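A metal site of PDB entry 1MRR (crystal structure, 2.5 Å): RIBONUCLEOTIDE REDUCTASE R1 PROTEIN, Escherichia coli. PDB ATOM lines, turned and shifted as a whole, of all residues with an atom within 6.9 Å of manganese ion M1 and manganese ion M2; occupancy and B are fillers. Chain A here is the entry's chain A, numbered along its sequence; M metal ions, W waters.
OE1 of Glu 204 lies close to NE1 of Trp 111.
The side-chain carboxylate of Glu 204 lies close to the side-chain amide nitrogen of Gln 87, at 3.3 Å.
The side-chain carboxylate (OE2) of Glu 115 sits close to the indole nitrogen (NE1) of Trp 111 (3.3 Å).
The side-chain hydroxyl (OH) of Tyr 122 sits at hydrogen-bond distance from the side-chain carboxylate (OD2) of Asp 84 (2.9 Å).
The backbone carbonyl oxygen (O) of Ser 114 lies close to a ring nitrogen (NE2) of His 118, 3.2 Å away.
A ring nitrogen (NE2) of His 118 lies within hydrogen-bond range of the side-chain carboxylate of Asp 237.
O of Asp 237 lies close to NE2 of His 241.
The backbone carbonyl oxygen (O) of Trp 111 lies within hydrogen-bond range of the side-chain hydroxyl (OG) of Ser 114, at 3.1 Å.
Four residues have an atom within 4 Å of manganese ion M1: Asp 84, Glu 115, His 118 and Glu 238.
The nearest printed residue that does not touch manganese ion M1 is Phe 208 (4.2 Å).
Trp 111 touches manganese ion M2 (NE1 to MN, 3.9 Å).
Within 4 Å of manganese ion M2: Trp 111, Glu 115, Glu 204, Glu 238 and His 241.
Manganese ion M1 is bound by OE2 of Glu 238 (2.1 Å), OD1 of Asp 84 (2.2 Å), OE1 of Glu 115 (2.2 Å) and ND1 of His 118 (2.3 Å).
Manganese ion M1 has four donor atoms within binding distance.
Slightly farther from manganese ion M1 lies water W1 (2.8 Å).
Slightly farther from manganese ion M1 lies the side-chain carboxylate (OD2) of Asp 84 (2.9 Å).
Manganese ion M2 is bound by OE1 of Glu 238, at 1.9 Å.
OE2 of Glu 204 binds manganese ion M2 (1.9 Å).
OE2 of Glu 115 is bound to manganese ion M2 (2.2 Å).
ND1 of His 241 is bound to manganese ion M2 (2.3 Å).
Water W1 binds manganese ion M2 (2.5 Å).
Slightly farther from manganese ion M2 lies the side-chain carboxylate (OE2) of Glu 238 (2.9 Å).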
ATOM      1  N   GLN A  80     -10.414 -27.606 -23.993  1.00  0.00           N
ATOM      2  CA  GLN A  80     -11.635 -27.246 -24.698  1.00  0.00           C
ATOM      3  C   GLN A  80     -11.419 -27.465 -26.190  1.00  0.00           C
ATOM      4  O   GLN A  80     -12.263 -28.089 -26.845  1.00  0.00           O
ATOM      5  CB  GLN A  80     -11.977 -25.781 -24.439  1.00  0.00           C
ATOM      6  CG  GLN A  80     -12.380 -25.494 -23.007  1.00  0.00           C
ATOM      7  CD  GLN A  80     -12.609 -24.035 -22.649  1.00  0.00           C
ATOM      8  OE1 GLN A  80     -12.020 -23.098 -23.189  1.00  0.00           O
ATOM      9  NE2 GLN A  80     -13.447 -23.748 -21.668  1.00  0.00           N
ATOM     10  N   LEU A  83     -11.603 -31.255 -27.008  1.00  0.00           N
ATOM     11  CA  LEU A  83     -12.939 -31.789 -27.007  1.00  0.00           C
ATOM     12  C   LEU A  83     -13.726 -31.317 -28.232  1.00  0.00           C
ATOM     13  O   LEU A  83     -14.298 -32.164 -28.925  1.00  0.00           O
ATOM     14  CB  LEU A  83     -13.662 -31.399 -25.686  1.00  0.00           C
ATOM     15  CG  LEU A  83     -13.146 -32.013 -24.363  1.00  0.00           C
ATOM     16  CD1 LEU A  83     -14.094 -31.656 -23.226  1.00  0.00           C
ATOM     17  CD2 LEU A  83     -13.058 -33.518 -24.475  1.00  0.00           C
ATOM     18  N   ASP A  84     -13.753 -30.002 -28.601  1.00  0.00           N
ATOM     19  CA  ASP A  84     -14.498 -29.627 -29.785  1.00  0.00           C
ATOM     20  C   ASP A  84     -13.908 -30.109 -31.087  1.00  0.00           C
ATOM     21  O   ASP A  84     -14.667 -30.349 -32.038  1.00  0.00           O
ATOM     22  CB  ASP A  84     -14.667 -28.164 -29.840  1.00  0.00           C
ATOM     23  CG  ASP A  84     -15.882 -27.728 -29.029  1.00  0.00           C
ATOM     24  OD1 ASP A  84     -16.929 -28.393 -29.076  1.00  0.00           O
ATOM     25  OD2 ASP A  84     -15.791 -26.692 -28.362  1.00  0.00           O
ATOM     26  N   GLN A  87     -15.626 -33.402 -31.200  1.00  0.00           N
ATOM     27  CA  GLN A  87     -17.073 -33.257 -31.331  1.00  0.00           C
ATOM     28  C   GLN A  87     -17.466 -32.671 -32.676  1.00  0.00           C
ATOM     29  O   GLN A  87     -18.624 -32.773 -33.054  1.00  0.00           O
ATOM     30  CB  GLN A  87     -17.626 -32.361 -30.217  1.00  0.00           C
ATOM     31  CG  GLN A  87     -17.626 -33.126 -28.899  1.00  0.00           C
ATOM     32  CD  GLN A  87     -18.578 -34.313 -28.912  1.00  0.00           C
ATOM     33  OE1 GLN A  87     -18.165 -35.452 -29.095  1.00  0.00           O
ATOM     34  NE2 GLN A  87     -19.889 -34.073 -28.765  1.00  0.00           N
ATOM     35  N   TRP A 111     -25.630 -30.157 -34.923  1.00  0.00           N
ATOM     36  CA  TRP A 111     -24.874 -30.279 -33.693  1.00  0.00           C
ATOM     37  C   TRP A 111     -23.378 -30.356 -34.035  1.00  0.00           C
ATOM     38  O   TRP A 111     -22.609 -29.597 -33.432  1.00  0.00           O
ATOM     39  CB  TRP A 111     -25.416 -31.536 -32.973  1.00  0.00           C
ATOM     40  CG  TRP A 111     -24.651 -32.085 -31.776  1.00  0.00           C
ATOM     41  CD1 TRP A 111     -23.733 -31.356 -31.058  1.00  0.00           C
ATOM     42  CD2 TRP A 111     -24.771 -33.360 -31.311  1.00  0.00           C
ATOM     43  NE1 TRP A 111     -23.272 -32.167 -30.144  1.00  0.00           N
ATOM     44  CE2 TRP A 111     -23.872 -33.368 -30.255  1.00  0.00           C
ATOM     45  CE3 TRP A 111     -25.528 -34.488 -31.628  1.00  0.00           C
ATOM     46  CZ2 TRP A 111     -23.701 -34.518 -29.506  1.00  0.00           C
ATOM     47  CZ3 TRP A 111     -25.361 -35.631 -30.875  1.00  0.00           C
ATOM     48  CH2 TRP A 111     -24.451 -35.638 -29.832  1.00  0.00           C
ATOM     49  N   SER A 114     -22.221 -26.749 -35.217  1.00  0.00           N
ATOM     50  CA  SER A 114     -21.933 -25.731 -34.198  1.00  0.00           C
ATOM     51  C   SER A 114     -20.634 -25.999 -33.403  1.00  0.00           C
ATOM     52  O   SER A 114     -20.039 -25.079 -32.826  1.00  0.00           O
ATOM     53  CB  SER A 114     -23.144 -25.654 -33.260  1.00  0.00           C
ATOM     54  OG  SER A 114     -23.309 -26.742 -32.362  1.00  0.00           O
ATOM     55  N   GLU A 115     -20.136 -27.247 -33.372  1.00  0.00           N
ATOM     56  CA  GLU A 115     -18.889 -27.565 -32.742  1.00  0.00           C
ATOM     57  C   GLU A 115     -17.777 -27.026 -33.599  1.00  0.00           C
ATOM     58  O   GLU A 115     -16.829 -26.491 -33.020  1.00  0.00           O
ATOM     59  CB  GLU A 115     -18.715 -29.066 -32.583  1.00  0.00           C
ATOM     60  CG  GLU A 115     -19.826 -29.778 -31.786  1.00  0.00           C
ATOM     61  CD  GLU A 115     -20.080 -29.433 -30.313  1.00  0.00           C
ATOM     62  OE1 GLU A 115     -19.777 -28.320 -29.837  1.00  0.00           O
ATOM     63  OE2 GLU A 115     -20.614 -30.320 -29.653  1.00  0.00           O
ATOM     64  N   THR A 116     -17.860 -27.011 -34.933  1.00  0.00           N
ATOM     65  CA  THR A 116     -16.755 -26.488 -35.719  1.00  0.00           C
ATOM     66  C   THR A 116     -16.667 -24.958 -35.518  1.00  0.00           C
ATOM     67  O   THR A 116     -15.583 -24.345 -35.575  1.00  0.00           O
ATOM     68  CB  THR A 116     -16.946 -26.920 -37.238  1.00  0.00           C
ATOM     69  OG1 THR A 116     -18.119 -26.361 -37.794  1.00  0.00           O
ATOM     70  CG2 THR A 116     -17.083 -28.436 -37.349  1.00  0.00           C
ATOM     71  N   HIS A 118     -17.176 -23.590 -32.614  1.00  0.00           N
ATOM     72  CA  HIS A 118     -16.510 -23.527 -31.303  1.00  0.00           C
ATOM     73  C   HIS A 118     -15.028 -23.686 -31.578  1.00  0.00           C
ATOM     74  O   HIS A 118     -14.261 -22.917 -31.047  1.00  0.00           O
ATOM     75  CB  HIS A 118     -17.023 -24.657 -30.395  1.00  0.00           C
ATOM     76  CG  HIS A 118     -18.524 -24.572 -30.049  1.00  0.00           C
ATOM     77  ND1 HIS A 118     -19.278 -25.459 -29.406  1.00  0.00           N
ATOM     78  CD2 HIS A 118     -19.326 -23.487 -30.357  1.00  0.00           C
ATOM     79  CE1 HIS A 118     -20.476 -24.949 -29.322  1.00  0.00           C
ATOM     80  NE2 HIS A 118     -20.492 -23.770 -29.890  1.00  0.00           N
ATOM     81  N   SER A 119     -14.603 -24.658 -32.373  1.00  0.00           N
ATOM     82  CA  SER A 119     -13.214 -24.761 -32.795  1.00  0.00           C
ATOM     83  C   SER A 119     -12.688 -23.433 -33.373  1.00  0.00           C
ATOM     84  O   SER A 119     -11.646 -22.944 -32.938  1.00  0.00           O
ATOM     85  CB  SER A 119     -13.073 -25.872 -33.838  1.00  0.00           C
ATOM     86  OG  SER A 119     -13.455 -27.107 -33.268  1.00  0.00           O
ATOM     87  N   TYR A 122     -11.852 -20.879 -30.753  1.00  0.00           N
ATOM     88  CA  TYR A 122     -10.608 -21.139 -30.067  1.00  0.00           C
ATOM     89  C   TYR A 122      -9.436 -20.627 -30.901  1.00  0.00           C
ATOM     90  O   TYR A 122      -8.555 -19.935 -30.356  1.00  0.00           O
ATOM     91  CB  TYR A 122     -10.484 -22.630 -29.786  1.00  0.00           C
ATOM     92  CG  TYR A 122     -11.591 -23.125 -28.858  1.00  0.00           C
ATOM     93  CD1 TYR A 122     -12.084 -22.364 -27.809  1.00  0.00           C
ATOM     94  CD2 TYR A 122     -12.132 -24.373 -29.107  1.00  0.00           C
ATOM     95  CE1 TYR A 122     -13.125 -22.856 -27.032  1.00  0.00           C
ATOM     96  CE2 TYR A 122     -13.172 -24.864 -28.331  1.00  0.00           C
ATOM     97  CZ  TYR A 122     -13.664 -24.103 -27.304  1.00  0.00           C
ATOM     98  OH  TYR A 122     -14.754 -24.602 -26.599  1.00  0.00           O
ATOM     99  N   LEU A 203     -19.431 -36.018 -21.503  1.00  0.00           N
ATOM    100  CA  LEU A 203     -18.547 -35.021 -22.102  1.00  0.00           C
ATOM    101  C   LEU A 203     -19.162 -33.647 -22.171  1.00  0.00           C
ATOM    102  O   LEU A 203     -18.563 -32.687 -21.666  1.00  0.00           O
ATOM    103  CB  LEU A 203     -18.116 -35.576 -23.504  1.00  0.00           C
ATOM    104  CG  LEU A 203     -17.736 -34.790 -24.803  1.00  0.00           C
ATOM    105  CD1 LEU A 203     -16.949 -33.576 -24.466  1.00  0.00           C
ATOM    106  CD2 LEU A 203     -16.865 -35.656 -25.718  1.00  0.00           C
ATOM    107  N   GLU A 204     -20.377 -33.533 -22.715  1.00  0.00           N
ATOM    108  CA  GLU A 204     -20.989 -32.215 -22.873  1.00  0.00           C
ATOM    109  C   GLU A 204     -21.580 -31.607 -21.618  1.00  0.00           C
ATOM    110  O   GLU A 204     -21.615 -30.382 -21.421  1.00  0.00           O
ATOM    111  CB  GLU A 204     -22.073 -32.263 -23.941  1.00  0.00           C
ATOM    112  CG  GLU A 204     -21.457 -32.815 -25.200  1.00  0.00           C
ATOM    113  CD  GLU A 204     -22.094 -32.336 -26.481  1.00  0.00           C
ATOM    114  OE1 GLU A 204     -23.219 -32.703 -26.753  1.00  0.00           O
ATOM    115  OE2 GLU A 204     -21.454 -31.599 -27.220  1.00  0.00           O
ATOM    116  N   PHE A 208     -17.358 -30.101 -20.167  1.00  0.00           N
ATOM    117  CA  PHE A 208     -17.308 -28.744 -20.652  1.00  0.00           C
ATOM    118  C   PHE A 208     -17.652 -27.809 -19.536  1.00  0.00           C
ATOM    119  O   PHE A 208     -17.048 -26.735 -19.423  1.00  0.00           O
ATOM    120  CB  PHE A 208     -18.276 -28.524 -21.829  1.00  0.00           C
ATOM    121  CG  PHE A 208     -17.481 -28.503 -23.137  1.00  0.00           C
ATOM    122  CD1 PHE A 208     -16.566 -27.482 -23.370  1.00  0.00           C
ATOM    123  CD2 PHE A 208     -17.592 -29.536 -24.061  1.00  0.00           C
ATOM    124  CE1 PHE A 208     -15.759 -27.484 -24.493  1.00  0.00           C
ATOM    125  CE2 PHE A 208     -16.775 -29.533 -25.183  1.00  0.00           C
ATOM    126  CZ  PHE A 208     -15.876 -28.509 -25.391  1.00  0.00           C
ATOM    127  N   PHE A 212     -15.767 -24.494 -18.285  1.00  0.00           N
ATOM    128  CA  PHE A 212     -16.439 -23.208 -18.303  1.00  0.00           C
ATOM    129  C   PHE A 212     -16.221 -22.482 -16.975  1.00  0.00           C
ATOM    130  O   PHE A 212     -15.947 -21.286 -16.974  1.00  0.00           O
ATOM    131  CB  PHE A 212     -17.944 -23.388 -18.523  1.00  0.00           C
ATOM    132  CG  PHE A 212     -18.389 -23.941 -19.862  1.00  0.00           C
ATOM    133  CD1 PHE A 212     -17.550 -23.960 -20.964  1.00  0.00           C
ATOM    134  CD2 PHE A 212     -19.678 -24.444 -19.966  1.00  0.00           C
ATOM    135  CE1 PHE A 212     -17.985 -24.488 -22.164  1.00  0.00           C
ATOM    136  CE2 PHE A 212     -20.119 -24.961 -21.171  1.00  0.00           C
ATOM    137  CZ  PHE A 212     -19.275 -24.987 -22.277  1.00  0.00           C
ATOM    138  N   ILE A 234     -20.634 -20.288 -26.333  1.00  0.00           N
ATOM    139  CA  ILE A 234     -20.385 -21.710 -26.439  1.00  0.00           C
ATOM    140  C   ILE A 234     -21.250 -22.465 -25.461  1.00  0.00           C
ATOM    141  O   ILE A 234     -21.886 -23.455 -25.852  1.00  0.00           O
ATOM    142  CB  ILE A 234     -18.886 -21.981 -26.172  1.00  0.00           C
ATOM    143  CG1 ILE A 234     -18.137 -21.454 -27.397  1.00  0.00           C
ATOM    144  CG2 ILE A 234     -18.596 -23.476 -25.910  1.00  0.00           C
ATOM    145  CD1 ILE A 234     -16.627 -21.775 -27.371  1.00  0.00           C
ATOM    146  N   ASP A 237     -24.750 -23.022 -26.410  1.00  0.00           N
ATOM    147  CA  ASP A 237     -24.966 -24.067 -27.387  1.00  0.00           C
ATOM    148  C   ASP A 237     -24.807 -25.409 -26.680  1.00  0.00           C
ATOM    149  O   ASP A 237     -25.550 -26.367 -26.963  1.00  0.00           O
ATOM    150  CB  ASP A 237     -23.965 -24.003 -28.505  1.00  0.00           C
ATOM    151  CG  ASP A 237     -24.056 -22.829 -29.455  1.00  0.00           C
ATOM    152  OD1 ASP A 237     -25.104 -22.208 -29.657  1.00  0.00           O
ATOM    153  OD2 ASP A 237     -23.032 -22.531 -30.023  1.00  0.00           O
ATOM    154  N   GLU A 238     -23.844 -25.570 -25.774  1.00  0.00           N
ATOM    155  CA  GLU A 238     -23.729 -26.838 -25.063  1.00  0.00           C
ATOM    156  C   GLU A 238     -24.991 -27.210 -24.287  1.00  0.00           C
ATOM    157  O   GLU A 238     -25.268 -28.409 -24.212  1.00  0.00           O
ATOM    158  CB  GLU A 238     -22.556 -26.848 -24.098  1.00  0.00           C
ATOM    159  CG  GLU A 238     -21.235 -26.744 -24.806  1.00  0.00           C
ATOM    160  CD  GLU A 238     -20.968 -27.656 -26.009  1.00  0.00           C
ATOM    161  OE1 GLU A 238     -21.386 -28.823 -26.018  1.00  0.00           O
ATOM    162  OE2 GLU A 238     -20.283 -27.194 -26.933  1.00  0.00           O
ATOM    163  N   ALA A 239     -25.768 -26.238 -23.793  1.00  0.00           N
ATOM    164  CA  ALA A 239     -27.044 -26.471 -23.155  1.00  0.00           C
ATOM    165  C   ALA A 239     -27.936 -27.300 -24.071  1.00  0.00           C
ATOM    166  O   ALA A 239     -28.496 -28.329 -23.693  1.00  0.00           O
ATOM    167  CB  ALA A 239     -27.809 -25.176 -22.903  1.00  0.00           C
ATOM    168  N   HIS A 241     -26.972 -29.101 -26.704  1.00  0.00           N
ATOM    169  CA  HIS A 241     -26.380 -30.382 -27.095  1.00  0.00           C
ATOM    170  C   HIS A 241     -26.639 -31.444 -26.062  1.00  0.00           C
ATOM    171  O   HIS A 241     -27.047 -32.552 -26.398  1.00  0.00           O
ATOM    172  CB  HIS A 241     -24.906 -30.199 -27.295  1.00  0.00           C
ATOM    173  CG  HIS A 241     -24.509 -29.189 -28.385  1.00  0.00           C
ATOM    174  ND1 HIS A 241     -23.282 -28.915 -28.812  1.00  0.00           N
ATOM    175  CD2 HIS A 241     -25.390 -28.415 -29.111  1.00  0.00           C
ATOM    176  CE1 HIS A 241     -23.404 -28.007 -29.756  1.00  0.00           C
ATOM    177  NE2 HIS A 241     -24.665 -27.720 -29.915  1.00  0.00           N
ATOM    178  N   LEU A 242     -26.507 -31.021 -24.798  1.00  0.00           N
ATOM    179  CA  LEU A 242     -26.784 -31.777 -23.582  1.00  0.00           C
ATOM    180  C   LEU A 242     -28.264 -32.186 -23.549  1.00  0.00           C
ATOM    181  O   LEU A 242     -28.606 -33.365 -23.390  1.00  0.00           O
ATOM    182  CB  LEU A 242     -26.409 -30.842 -22.447  1.00  0.00           C
ATOM    183  CG  LEU A 242     -26.685 -30.859 -20.943  1.00  0.00           C
ATOM    184  CD1 LEU A 242     -25.822 -29.721 -20.389  1.00  0.00           C
ATOM    185  CD2 LEU A 242     -28.107 -30.518 -20.550  1.00  0.00           C
HETATM  186 MN    MN M   1     -18.638 -27.296 -28.251  1.00  0.00          MN
HETATM  187 MN    MN M   2     -21.416 -29.727 -27.723  1.00  0.00          MN
HETATM  188  O   HOH W   1     -18.912 -29.937 -27.385  1.00  0.00           O
